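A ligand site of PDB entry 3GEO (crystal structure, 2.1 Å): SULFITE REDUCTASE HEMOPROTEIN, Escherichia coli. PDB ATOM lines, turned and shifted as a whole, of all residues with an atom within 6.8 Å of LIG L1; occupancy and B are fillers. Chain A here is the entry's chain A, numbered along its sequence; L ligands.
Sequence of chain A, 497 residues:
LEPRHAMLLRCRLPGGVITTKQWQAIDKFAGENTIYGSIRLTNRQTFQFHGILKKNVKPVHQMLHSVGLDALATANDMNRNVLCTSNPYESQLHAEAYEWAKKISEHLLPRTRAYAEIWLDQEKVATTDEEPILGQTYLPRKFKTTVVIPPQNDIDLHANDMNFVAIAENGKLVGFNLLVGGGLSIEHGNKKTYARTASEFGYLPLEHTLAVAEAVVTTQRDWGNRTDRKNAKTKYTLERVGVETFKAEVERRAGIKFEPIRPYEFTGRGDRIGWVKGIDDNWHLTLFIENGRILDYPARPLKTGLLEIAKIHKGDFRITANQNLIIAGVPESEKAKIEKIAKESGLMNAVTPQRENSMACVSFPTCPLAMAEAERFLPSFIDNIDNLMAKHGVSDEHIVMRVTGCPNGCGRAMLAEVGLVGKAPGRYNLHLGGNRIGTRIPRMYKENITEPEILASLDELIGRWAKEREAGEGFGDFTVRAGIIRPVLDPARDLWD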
ATOM      1  N   ALA A 360       8.103 -13.834 -24.180  1.00  0.00           N
ATOM      2  CA  ALA A 360       8.582 -14.290 -25.484  1.00  0.00           C
ATOM      3  C   ALA A 360      10.103 -14.479 -25.445  1.00  0.00           C
ATOM      4  O   ALA A 360      10.778 -13.866 -24.617  1.00  0.00           O
ATOM      5  CB  ALA A 360       8.200 -13.275 -26.569  1.00  0.00           C
ATOM      6  N   CYS A 361      10.637 -15.387 -26.267  1.00  0.00           N
ATOM      7  CA  CYS A 361      12.085 -15.587 -26.335  1.00  0.00           C
ATOM      8  C   CYS A 361      12.695 -14.536 -27.295  1.00  0.00           C
ATOM      9  O   CYS A 361      11.970 -13.815 -28.001  1.00  0.00           O
ATOM     10  CB  CYS A 361      12.438 -16.972 -26.869  1.00  0.00           C
ATOM     11  SG  CYS A 361      12.031 -17.086 -28.636  1.00  0.00           S
ATOM     12  N   VAL A 362      14.013 -14.489 -27.343  1.00  0.00           N
ATOM     13  CA  VAL A 362      14.750 -13.544 -28.212  1.00  0.00           C
ATOM     14  C   VAL A 362      14.378 -13.650 -29.715  1.00  0.00           C
ATOM     15  O   VAL A 362      13.922 -12.661 -30.331  1.00  0.00           O
ATOM     16  CB  VAL A 362      16.277 -13.721 -28.053  1.00  0.00           C
ATOM     17  CG1 VAL A 362      17.015 -12.865 -29.065  1.00  0.00           C
ATOM     18  CG2 VAL A 362      16.682 -13.389 -26.617  1.00  0.00           C
ATOM     19  N   SER A 363      14.564 -14.840 -30.276  1.00  0.00           N
ATOM     20  CA  SER A 363      14.253 -15.080 -31.685  1.00  0.00           C
ATOM     21  C   SER A 363      15.060 -14.129 -32.602  1.00  0.00           C
ATOM     22  O   SER A 363      16.248 -13.903 -32.369  1.00  0.00           O
ATOM     23  CB  SER A 363      12.732 -14.933 -31.887  1.00  0.00           C
ATOM     24  OG  SER A 363      12.360 -15.339 -33.183  1.00  0.00           O
ATOM     25  N   PHE A 364      14.428 -13.601 -33.650  1.00  0.00           N
ATOM     26  CA  PHE A 364      15.079 -12.665 -34.564  1.00  0.00           C
ATOM     27  C   PHE A 364      15.287 -11.352 -33.807  1.00  0.00           C
ATOM     28  O   PHE A 364      14.417 -10.955 -33.024  1.00  0.00           O
ATOM     29  CB  PHE A 364      14.198 -12.358 -35.782  1.00  0.00           C
ATOM     30  CG  PHE A 364      13.902 -13.541 -36.650  1.00  0.00           C
ATOM     31  CD1 PHE A 364      14.934 -14.219 -37.274  1.00  0.00           C
ATOM     32  CD2 PHE A 364      12.595 -13.959 -36.867  1.00  0.00           C
ATOM     33  CE1 PHE A 364      14.656 -15.312 -38.105  1.00  0.00           C
ATOM     34  CE2 PHE A 364      12.299 -15.039 -37.686  1.00  0.00           C
ATOM     35  CZ  PHE A 364      13.331 -15.718 -38.309  1.00  0.00           C
ATOM     36  N   CYS A 367      18.863 -14.655 -33.102  1.00  0.00           N
ATOM     37  CA  CYS A 367      18.885 -16.095 -33.046  1.00  0.00           C
ATOM     38  C   CYS A 367      18.942 -16.744 -34.439  1.00  0.00           C
ATOM     39  O   CYS A 367      18.234 -16.345 -35.360  1.00  0.00           O
ATOM     40  CB  CYS A 367      17.709 -16.643 -32.256  1.00  0.00           C
ATOM     41  SG  CYS A 367      17.906 -18.411 -31.906  1.00  0.00           S
ATOM     42  N   PRO A 368      19.826 -17.733 -34.607  1.00  0.00           N
ATOM     43  CA  PRO A 368      19.989 -18.445 -35.876  1.00  0.00           C
ATOM     44  C   PRO A 368      18.945 -19.571 -36.125  1.00  0.00           C
ATOM     45  O   PRO A 368      18.736 -20.002 -37.272  1.00  0.00           O
ATOM     46  CB  PRO A 368      21.399 -19.019 -35.753  1.00  0.00           C
ATOM     47  CG  PRO A 368      21.518 -19.306 -34.253  1.00  0.00           C
ATOM     48  CD  PRO A 368      20.909 -18.057 -33.655  1.00  0.00           C
ATOM     49  N   LEU A 369      18.304 -20.012 -35.055  1.00  0.00           N
ATOM     50  CA  LEU A 369      17.314 -21.088 -35.107  1.00  0.00           C
ATOM     51  C   LEU A 369      15.916 -20.545 -35.180  1.00  0.00           C
ATOM     52  O   LEU A 369      14.938 -21.293 -35.188  1.00  0.00           O
ATOM     53  CB  LEU A 369      17.434 -21.948 -33.862  1.00  0.00           C
ATOM     54  CG  LEU A 369      18.888 -22.364 -33.621  1.00  0.00           C
ATOM     55  CD1 LEU A 369      18.990 -23.155 -32.342  1.00  0.00           C
ATOM     56  CD2 LEU A 369      19.388 -23.162 -34.819  1.00  0.00           C
ATOM     57  N   ALA A 370      15.808 -19.220 -35.195  1.00  0.00           N
ATOM     58  CA  ALA A 370      14.498 -18.605 -35.235  1.00  0.00           C
ATOM     59  C   ALA A 370      13.729 -18.948 -36.522  1.00  0.00           C
ATOM     60  O   ALA A 370      14.294 -18.943 -37.612  1.00  0.00           O
ATOM     61  CB  ALA A 370      14.619 -17.110 -35.056  1.00  0.00           C
ATOM     62  N   MET A 371      12.447 -19.228 -36.360  1.00  0.00           N
ATOM     63  CA  MET A 371      11.562 -19.535 -37.484  1.00  0.00           C
ATOM     64  C   MET A 371      10.547 -18.400 -37.637  1.00  0.00           C
ATOM     65  O   MET A 371      10.118 -18.071 -38.735  1.00  0.00           O
ATOM     66  CB  MET A 371      10.836 -20.857 -37.235  1.00  0.00           C
ATOM     67  CG  MET A 371      11.777 -22.041 -37.052  1.00  0.00           C
ATOM     68  SD  MET A 371      10.890 -23.570 -36.649  1.00  0.00           S
ATOM     69  CE  MET A 371      11.949 -24.863 -37.415  1.00  0.00           C
ATOM     70  N   ALA A 372      10.150 -17.806 -36.517  1.00  0.00           N
ATOM     71  CA  ALA A 372       9.188 -16.720 -36.512  1.00  0.00           C
ATOM     72  C   ALA A 372       9.607 -15.739 -35.415  1.00  0.00           C
ATOM     73  O   ALA A 372      10.433 -16.066 -34.575  1.00  0.00           O
ATOM     74  CB  ALA A 372       7.801 -17.251 -36.251  1.00  0.00           C
ATOM     75  N   ALA A 374       9.486 -13.397 -32.090  1.00  0.00           N
ATOM     76  CA  ALA A 374       9.041 -13.672 -30.746  1.00  0.00           C
ATOM     77  C   ALA A 374       9.152 -12.354 -29.998  1.00  0.00           C
ATOM     78  O   ALA A 374       8.171 -11.608 -29.910  1.00  0.00           O
ATOM     79  CB  ALA A 374       9.899 -14.737 -30.143  1.00  0.00           C
ATOM     80  N   VAL A 403       5.257 -16.845 -26.280  1.00  0.00           N
ATOM     81  CA  VAL A 403       5.601 -17.037 -27.674  1.00  0.00           C
ATOM     82  C   VAL A 403       7.026 -17.486 -27.752  1.00  0.00           C
ATOM     83  O   VAL A 403       7.915 -16.827 -27.256  1.00  0.00           O
ATOM     84  CB  VAL A 403       5.489 -15.723 -28.434  1.00  0.00           C
ATOM     85  CG1 VAL A 403       5.852 -15.935 -29.904  1.00  0.00           C
ATOM     86  CG2 VAL A 403       4.084 -15.141 -28.301  1.00  0.00           C
ATOM     87  N   THR A 404       7.236 -18.649 -28.316  1.00  0.00           N
ATOM     88  CA  THR A 404       8.594 -19.142 -28.476  1.00  0.00           C
ATOM     89  C   THR A 404       8.893 -19.095 -30.011  1.00  0.00           C
ATOM     90  O   THR A 404       8.045 -19.451 -30.825  1.00  0.00           O
ATOM     91  CB  THR A 404       8.764 -20.552 -27.806  1.00  0.00           C
ATOM     92  OG1 THR A 404      10.155 -20.867 -27.701  1.00  0.00           O
ATOM     93  CG2 THR A 404       8.018 -21.657 -28.508  1.00  0.00           C
ATOM     94  N   GLY A 405      10.029 -18.494 -30.377  1.00  0.00           N
ATOM     95  CA  GLY A 405      10.400 -18.351 -31.770  1.00  0.00           C
ATOM     96  C   GLY A 405      10.559 -19.593 -32.621  1.00  0.00           C
ATOM     97  O   GLY A 405      10.467 -19.533 -33.846  1.00  0.00           O
ATOM     98  N   CYS A 406      10.814 -20.732 -31.974  1.00  0.00           N
ATOM     99  CA  CYS A 406      10.964 -22.001 -32.661  1.00  0.00           C
ATOM    100  C   CYS A 406      10.725 -23.095 -31.603  1.00  0.00           C
ATOM    101  O   CYS A 406      10.757 -22.801 -30.412  1.00  0.00           O
ATOM    102  CB  CYS A 406      12.351 -22.089 -33.327  1.00  0.00           C
ATOM    103  SG  CYS A 406      13.676 -22.690 -32.249  1.00  0.00           S
ATOM    104  N   PRO A 407      10.464 -24.337 -32.013  1.00  0.00           N
ATOM    105  CA  PRO A 407      10.204 -25.470 -31.125  1.00  0.00           C
ATOM    106  C   PRO A 407      11.210 -25.807 -30.014  1.00  0.00           C
ATOM    107  O   PRO A 407      10.890 -26.588 -29.092  1.00  0.00           O
ATOM    108  CB  PRO A 407       9.947 -26.622 -32.094  1.00  0.00           C
ATOM    109  CG  PRO A 407      10.788 -26.252 -33.253  1.00  0.00           C
ATOM    110  CD  PRO A 407      10.447 -24.793 -33.414  1.00  0.00           C
ATOM    111  N   ASN A 408      12.410 -25.218 -30.053  1.00  0.00           N
ATOM    112  CA  ASN A 408      13.399 -25.446 -28.990  1.00  0.00           C
ATOM    113  C   ASN A 408      12.715 -25.064 -27.663  1.00  0.00           C
ATOM    114  O   ASN A 408      13.005 -25.629 -26.605  1.00  0.00           O
ATOM    115  CB  ASN A 408      14.679 -24.617 -29.210  1.00  0.00           C
ATOM    116  CG  ASN A 408      15.571 -25.220 -30.275  1.00  0.00           C
ATOM    117  OD1 ASN A 408      15.659 -26.443 -30.395  1.00  0.00           O
ATOM    118  ND2 ASN A 408      16.236 -24.364 -31.053  1.00  0.00           N
ATOM    119  N   GLY A 409      11.783 -24.116 -27.750  1.00  0.00           N
ATOM    120  CA  GLY A 409      10.997 -23.711 -26.609  1.00  0.00           C
ATOM    121  C   GLY A 409      11.577 -22.764 -25.573  1.00  0.00           C
ATOM    122  O   GLY A 409      11.155 -22.850 -24.418  1.00  0.00           O
ATOM    123  N   CYS A 410      12.435 -21.821 -25.979  1.00  0.00           N
ATOM    124  CA  CYS A 410      13.025 -20.896 -25.020  1.00  0.00           C
ATOM    125  C   CYS A 410      12.067 -19.960 -24.273  1.00  0.00           C
ATOM    126  O   CYS A 410      12.281 -19.646 -23.113  1.00  0.00           O
ATOM    127  CB  CYS A 410      14.126 -20.099 -25.674  1.00  0.00           C
ATOM    128  SG  CYS A 410      15.309 -21.222 -26.434  1.00  0.00           S
ATOM    129  N   GLY A 411      11.002 -19.548 -24.951  1.00  0.00           N
ATOM    130  CA  GLY A 411      10.029 -18.656 -24.338  1.00  0.00           C
ATOM    131  C   GLY A 411       9.040 -19.348 -23.422  1.00  0.00           C
ATOM    132  O   GLY A 411       8.099 -18.704 -22.947  1.00  0.00           O
HETATM  133 FE1  LIG L   1      13.501 -18.565 -29.560  1.00  0.00          FE
HETATM  134 FE2  LIG L   1      15.974 -18.970 -30.807  1.00  0.00          FE
HETATM  135 FE3  LIG L   1      14.093 -20.842 -30.967  1.00  0.00          FE
HETATM  136 FE4  LIG L   1      15.169 -20.264 -28.472  1.00  0.00          FE
HETATM  137  S1  LIG L   1      16.294 -21.184 -30.313  1.00  0.00           S
HETATM  138  S2  LIG L   1      13.032 -20.719 -28.951  1.00  0.00           S
HETATM  139  S3  LIG L   1      15.455 -17.966 -28.746  1.00  0.00           S
HETATM  140  S4  LIG L   1      13.964 -18.717 -31.826  1.00  0.00           S
HETATM  141 FE1  LG2 L   2      17.348 -21.272 -25.117  1.00  0.00          FE
HETATM  142  C1  LG2 L   2      19.227 -22.368 -27.740  1.00  0.00           C
HETATM  143  C2  LG2 L   2      17.911 -18.076 -25.993  1.00  0.00           C
HETATM  144  C3  LG2 L   2      15.841 -20.237 -22.244  1.00  0.00           C
HETATM  145  C4  LG2 L   2      15.878 -24.315 -24.782  1.00  0.00           C
HETATM  146  N1  LG2 L   2      18.527 -20.352 -26.566  1.00  0.00           N
HETATM  147  C5  LG2 L   2      19.257 -21.004 -27.527  1.00  0.00           C
HETATM  148  C6  LG2 L   2      20.197 -19.976 -28.132  1.00  0.00           C
HETATM  149  C7  LG2 L   2      21.396 -19.926 -27.145  1.00  0.00           C
HETATM  150  C8  LG2 L   2      20.527 -20.193 -29.643  1.00  0.00           C
HETATM  151  C9  LG2 L   2      21.742 -21.039 -30.022  1.00  0.00           C
HETATM  152  O1  LG2 L   2      21.704 -22.264 -29.789  1.00  0.00           O
HETATM  153  O2  LG2 L   2      22.736 -20.477 -30.539  1.00  0.00           O
HETATM  154  C10 LG2 L   2      19.261 -18.797 -28.087  1.00  0.00           C
HETATM  155  C11 LG2 L   2      20.003 -17.517 -28.170  1.00  0.00           C
HETATM  156  C12 LG2 L   2      19.179 -16.406 -28.813  1.00  0.00           C
HETATM  157  C13 LG2 L   2      19.901 -15.079 -28.808  1.00  0.00           C
HETATM  158  O3  LG2 L   2      20.193 -14.570 -29.911  1.00  0.00           O
HETATM  159  O4  LG2 L   2      20.170 -14.545 -27.716  1.00  0.00           O
HETATM  160  C14 LG2 L   2      18.568 -19.028 -26.758  1.00  0.00           C
HETATM  161  N2  LG2 L   2      16.902 -19.452 -24.280  1.00  0.00           N
HETATM  162  C15 LG2 L   2      17.142 -18.255 -24.875  1.00  0.00           C
HETATM  163  C16 LG2 L   2      16.664 -17.157 -23.943  1.00  0.00           C
HETATM  164  C17 LG2 L   2      17.648 -15.978 -24.056  1.00  0.00           C
HETATM  165  C18 LG2 L   2      15.170 -16.858 -24.341  1.00  0.00           C
HETATM  166  C19 LG2 L   2      14.618 -15.621 -23.677  1.00  0.00           C
HETATM  167  O5  LG2 L   2      14.138 -14.736 -24.383  1.00  0.00           O
HETATM  168  O6  LG2 L   2      14.676 -15.518 -22.448  1.00  0.00           O
HETATM  169  C20 LG2 L   2      16.858 -17.892 -22.568  1.00  0.00           C
HETATM  170  C21 LG2 L   2      18.304 -17.924 -22.156  1.00  0.00           C
HETATM  171  C22 LG2 L   2      18.535 -18.898 -21.022  1.00  0.00           C
HETATM  172  C23 LG2 L   2      19.863 -18.702 -20.322  1.00  0.00           C
HETATM  173  O7  LG2 L   2      20.233 -17.535 -20.084  1.00  0.00           O
HETATM  174  O8  LG2 L   2      20.547 -19.698 -20.012  1.00  0.00           O
HETATM  175  C24 LG2 L   2      16.392 -19.264 -23.024  1.00  0.00           C
HETATM  176  N3  LG2 L   2      16.081 -22.125 -23.721  1.00  0.00           N
HETATM  177  C25 LG2 L   2      15.664 -21.553 -22.566  1.00  0.00           C
HETATM  178  C26 LG2 L   2      14.471 -22.343 -22.065  1.00  0.00           C
HETATM  179  C27 LG2 L   2      13.666 -21.875 -20.877  1.00  0.00           C
HETATM  180  C28 LG2 L   2      14.357 -22.094 -19.539  1.00  0.00           C
HETATM  181  O9  LG2 L   2      15.498 -22.611 -19.511  1.00  0.00           O
HETATM  182  O10 LG2 L   2      13.770 -21.741 -18.518  1.00  0.00           O
HETATM  183  C29 LG2 L   2      14.369 -23.487 -22.834  1.00  0.00           C
HETATM  184  C30 LG2 L   2      13.331 -24.594 -22.731  1.00  0.00           C
HETATM  185  C31 LG2 L   2      13.553 -25.668 -21.662  1.00  0.00           C
HETATM  186  C32 LG2 L   2      14.490 -26.790 -22.119  1.00  0.00           C
HETATM  187  O11 LG2 L   2      15.693 -26.548 -22.246  1.00  0.00           O
HETATM  188  O12 LG2 L   2      14.008 -27.926 -22.326  1.00  0.00           O
HETATM  189  C33 LG2 L   2      15.478 -23.356 -23.850  1.00  0.00           C
HETATM  190  N4  LG2 L   2      17.628 -23.094 -26.039  1.00  0.00           N
HETATM  191  C34 LG2 L   2      16.870 -24.206 -25.759  1.00  0.00           C
HETATM  192  C35 LG2 L   2      17.237 -25.234 -26.797  1.00  0.00           C
HETATM  193  C36 LG2 L   2      16.597 -26.593 -26.842  1.00  0.00           C
HETATM  194  C37 LG2 L   2      17.277 -27.542 -25.871  1.00  0.00           C
HETATM  195  C38 LG2 L   2      16.894 -28.987 -26.116  1.00  0.00           C
HETATM  196  O13 LG2 L   2      16.867 -29.774 -25.147  1.00  0.00           O
HETATM  197  O14 LG2 L   2      16.643 -29.347 -27.281  1.00  0.00           O
HETATM  198  C39 LG2 L   2      18.196 -24.678 -27.646  1.00  0.00           C
HETATM  199  C40 LG2 L   2      18.922 -25.219 -28.853  1.00  0.00           C
HETATM  200  C41 LG2 L   2      19.888 -26.232 -28.294  1.00  0.00           C
HETATM  201  O15 LG2 L   2      20.780 -25.827 -27.519  1.00  0.00           O
HETATM  202  O16 LG2 L   2      19.752 -27.421 -28.608  1.00  0.00           O
HETATM  203  C42 LG2 L   2      18.490 -23.325 -27.091  1.00  0.00           C
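N of Cys 410 sits at hydrogen-bond distance from OG1 of Thr 404, at 3.0 Å.
The side-chain sulfur (SG) of Cys 361 sits close to the backbone NH (N) of Gly 405 (3.0 Å).
The backbone carbonyl oxygen (O) of Val 403 lies within hydrogen-bond range of the backbone NH (N) of Cys 361.
The backbone carbonyl oxygen of Cys 406 is in hydrogen-bond range of the side-chain hydroxyl of Thr 404, 3.4 Å away.
The side-chain sulfur of Cys 406 sits close to the side-chain amide nitrogen of Asn 408 (3.3 Å).
The side-chain sulfur (SG) of Cys 367 sits close to the backbone NH (N) of Leu 369.
N of Met 371 is in hydrogen-bond range of O of Gly 405 (3.2 Å).
OG of Ser 363 lies within hydrogen-bond range of O of Ala 372 (2.5 Å).
N of Cys 410 lies close to S2 of LIG L1 (3.2 Å).
An iron atom (FE4) of LIG L1 is bound by the side-chain sulfur (SG) of Cys 410 (2.3 Å).
SG of Cys 361 is bound to FE1 of LIG L1 (2.3 Å).
The backbone NH of Cys 406 sits close to a sulfur (S4) of LIG L1 (3.7 Å).
SG of Cys 406 binds FE3 of LIG L1, at 2.3 Å.
The side-chain sulfur of Cys 367 binds an iron atom (FE2) of LIG L1 (2.3 Å).
The side-chain hydroxyl of Thr 404 lies close to a sulfur (S2) of LIG L1.
The side-chain amide nitrogen (ND2) of Asn 408 lies close to a sulfur (S1) of LIG L1 (3.3 Å).
A sulfur (S3) of LIG L1 lies close to the backbone NH (N) of Ser 363.
An iron atom (FE1) of LG2 L2 is bound by the side-chain sulfur (SG) of Cys 410.
An oxygen (O3) of LG2 L2 is in hydrogen-bond range of the backbone NH (N) of Cys 367 (3.5 Å).
The backbone NH of Val 362 lies within hydrogen-bond range of an oxygen (O5) of LG2 L2 (3.0 Å).
Merely in contact with LIG L1: Ala 370 (3.5 Å), Gly 405 (3.6 Å), Leu 369 (3.8 Å) and Gly 409 (3.8 Å).
Hydrophobic or aromatic side chains within 4 Å of LIG L1: Leu 369 and Ala 370.
Within 4 Å of LIG L1: Cys 361, Ser 363, Cys 367, Leu 369, Ala 370, Thr 404, Gly 405, Cys 406, Asn 408, Gly 409 and Cys 410.
The nearest printed residue that does not touch LIG L1 is Val 362 (4.02 Å).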
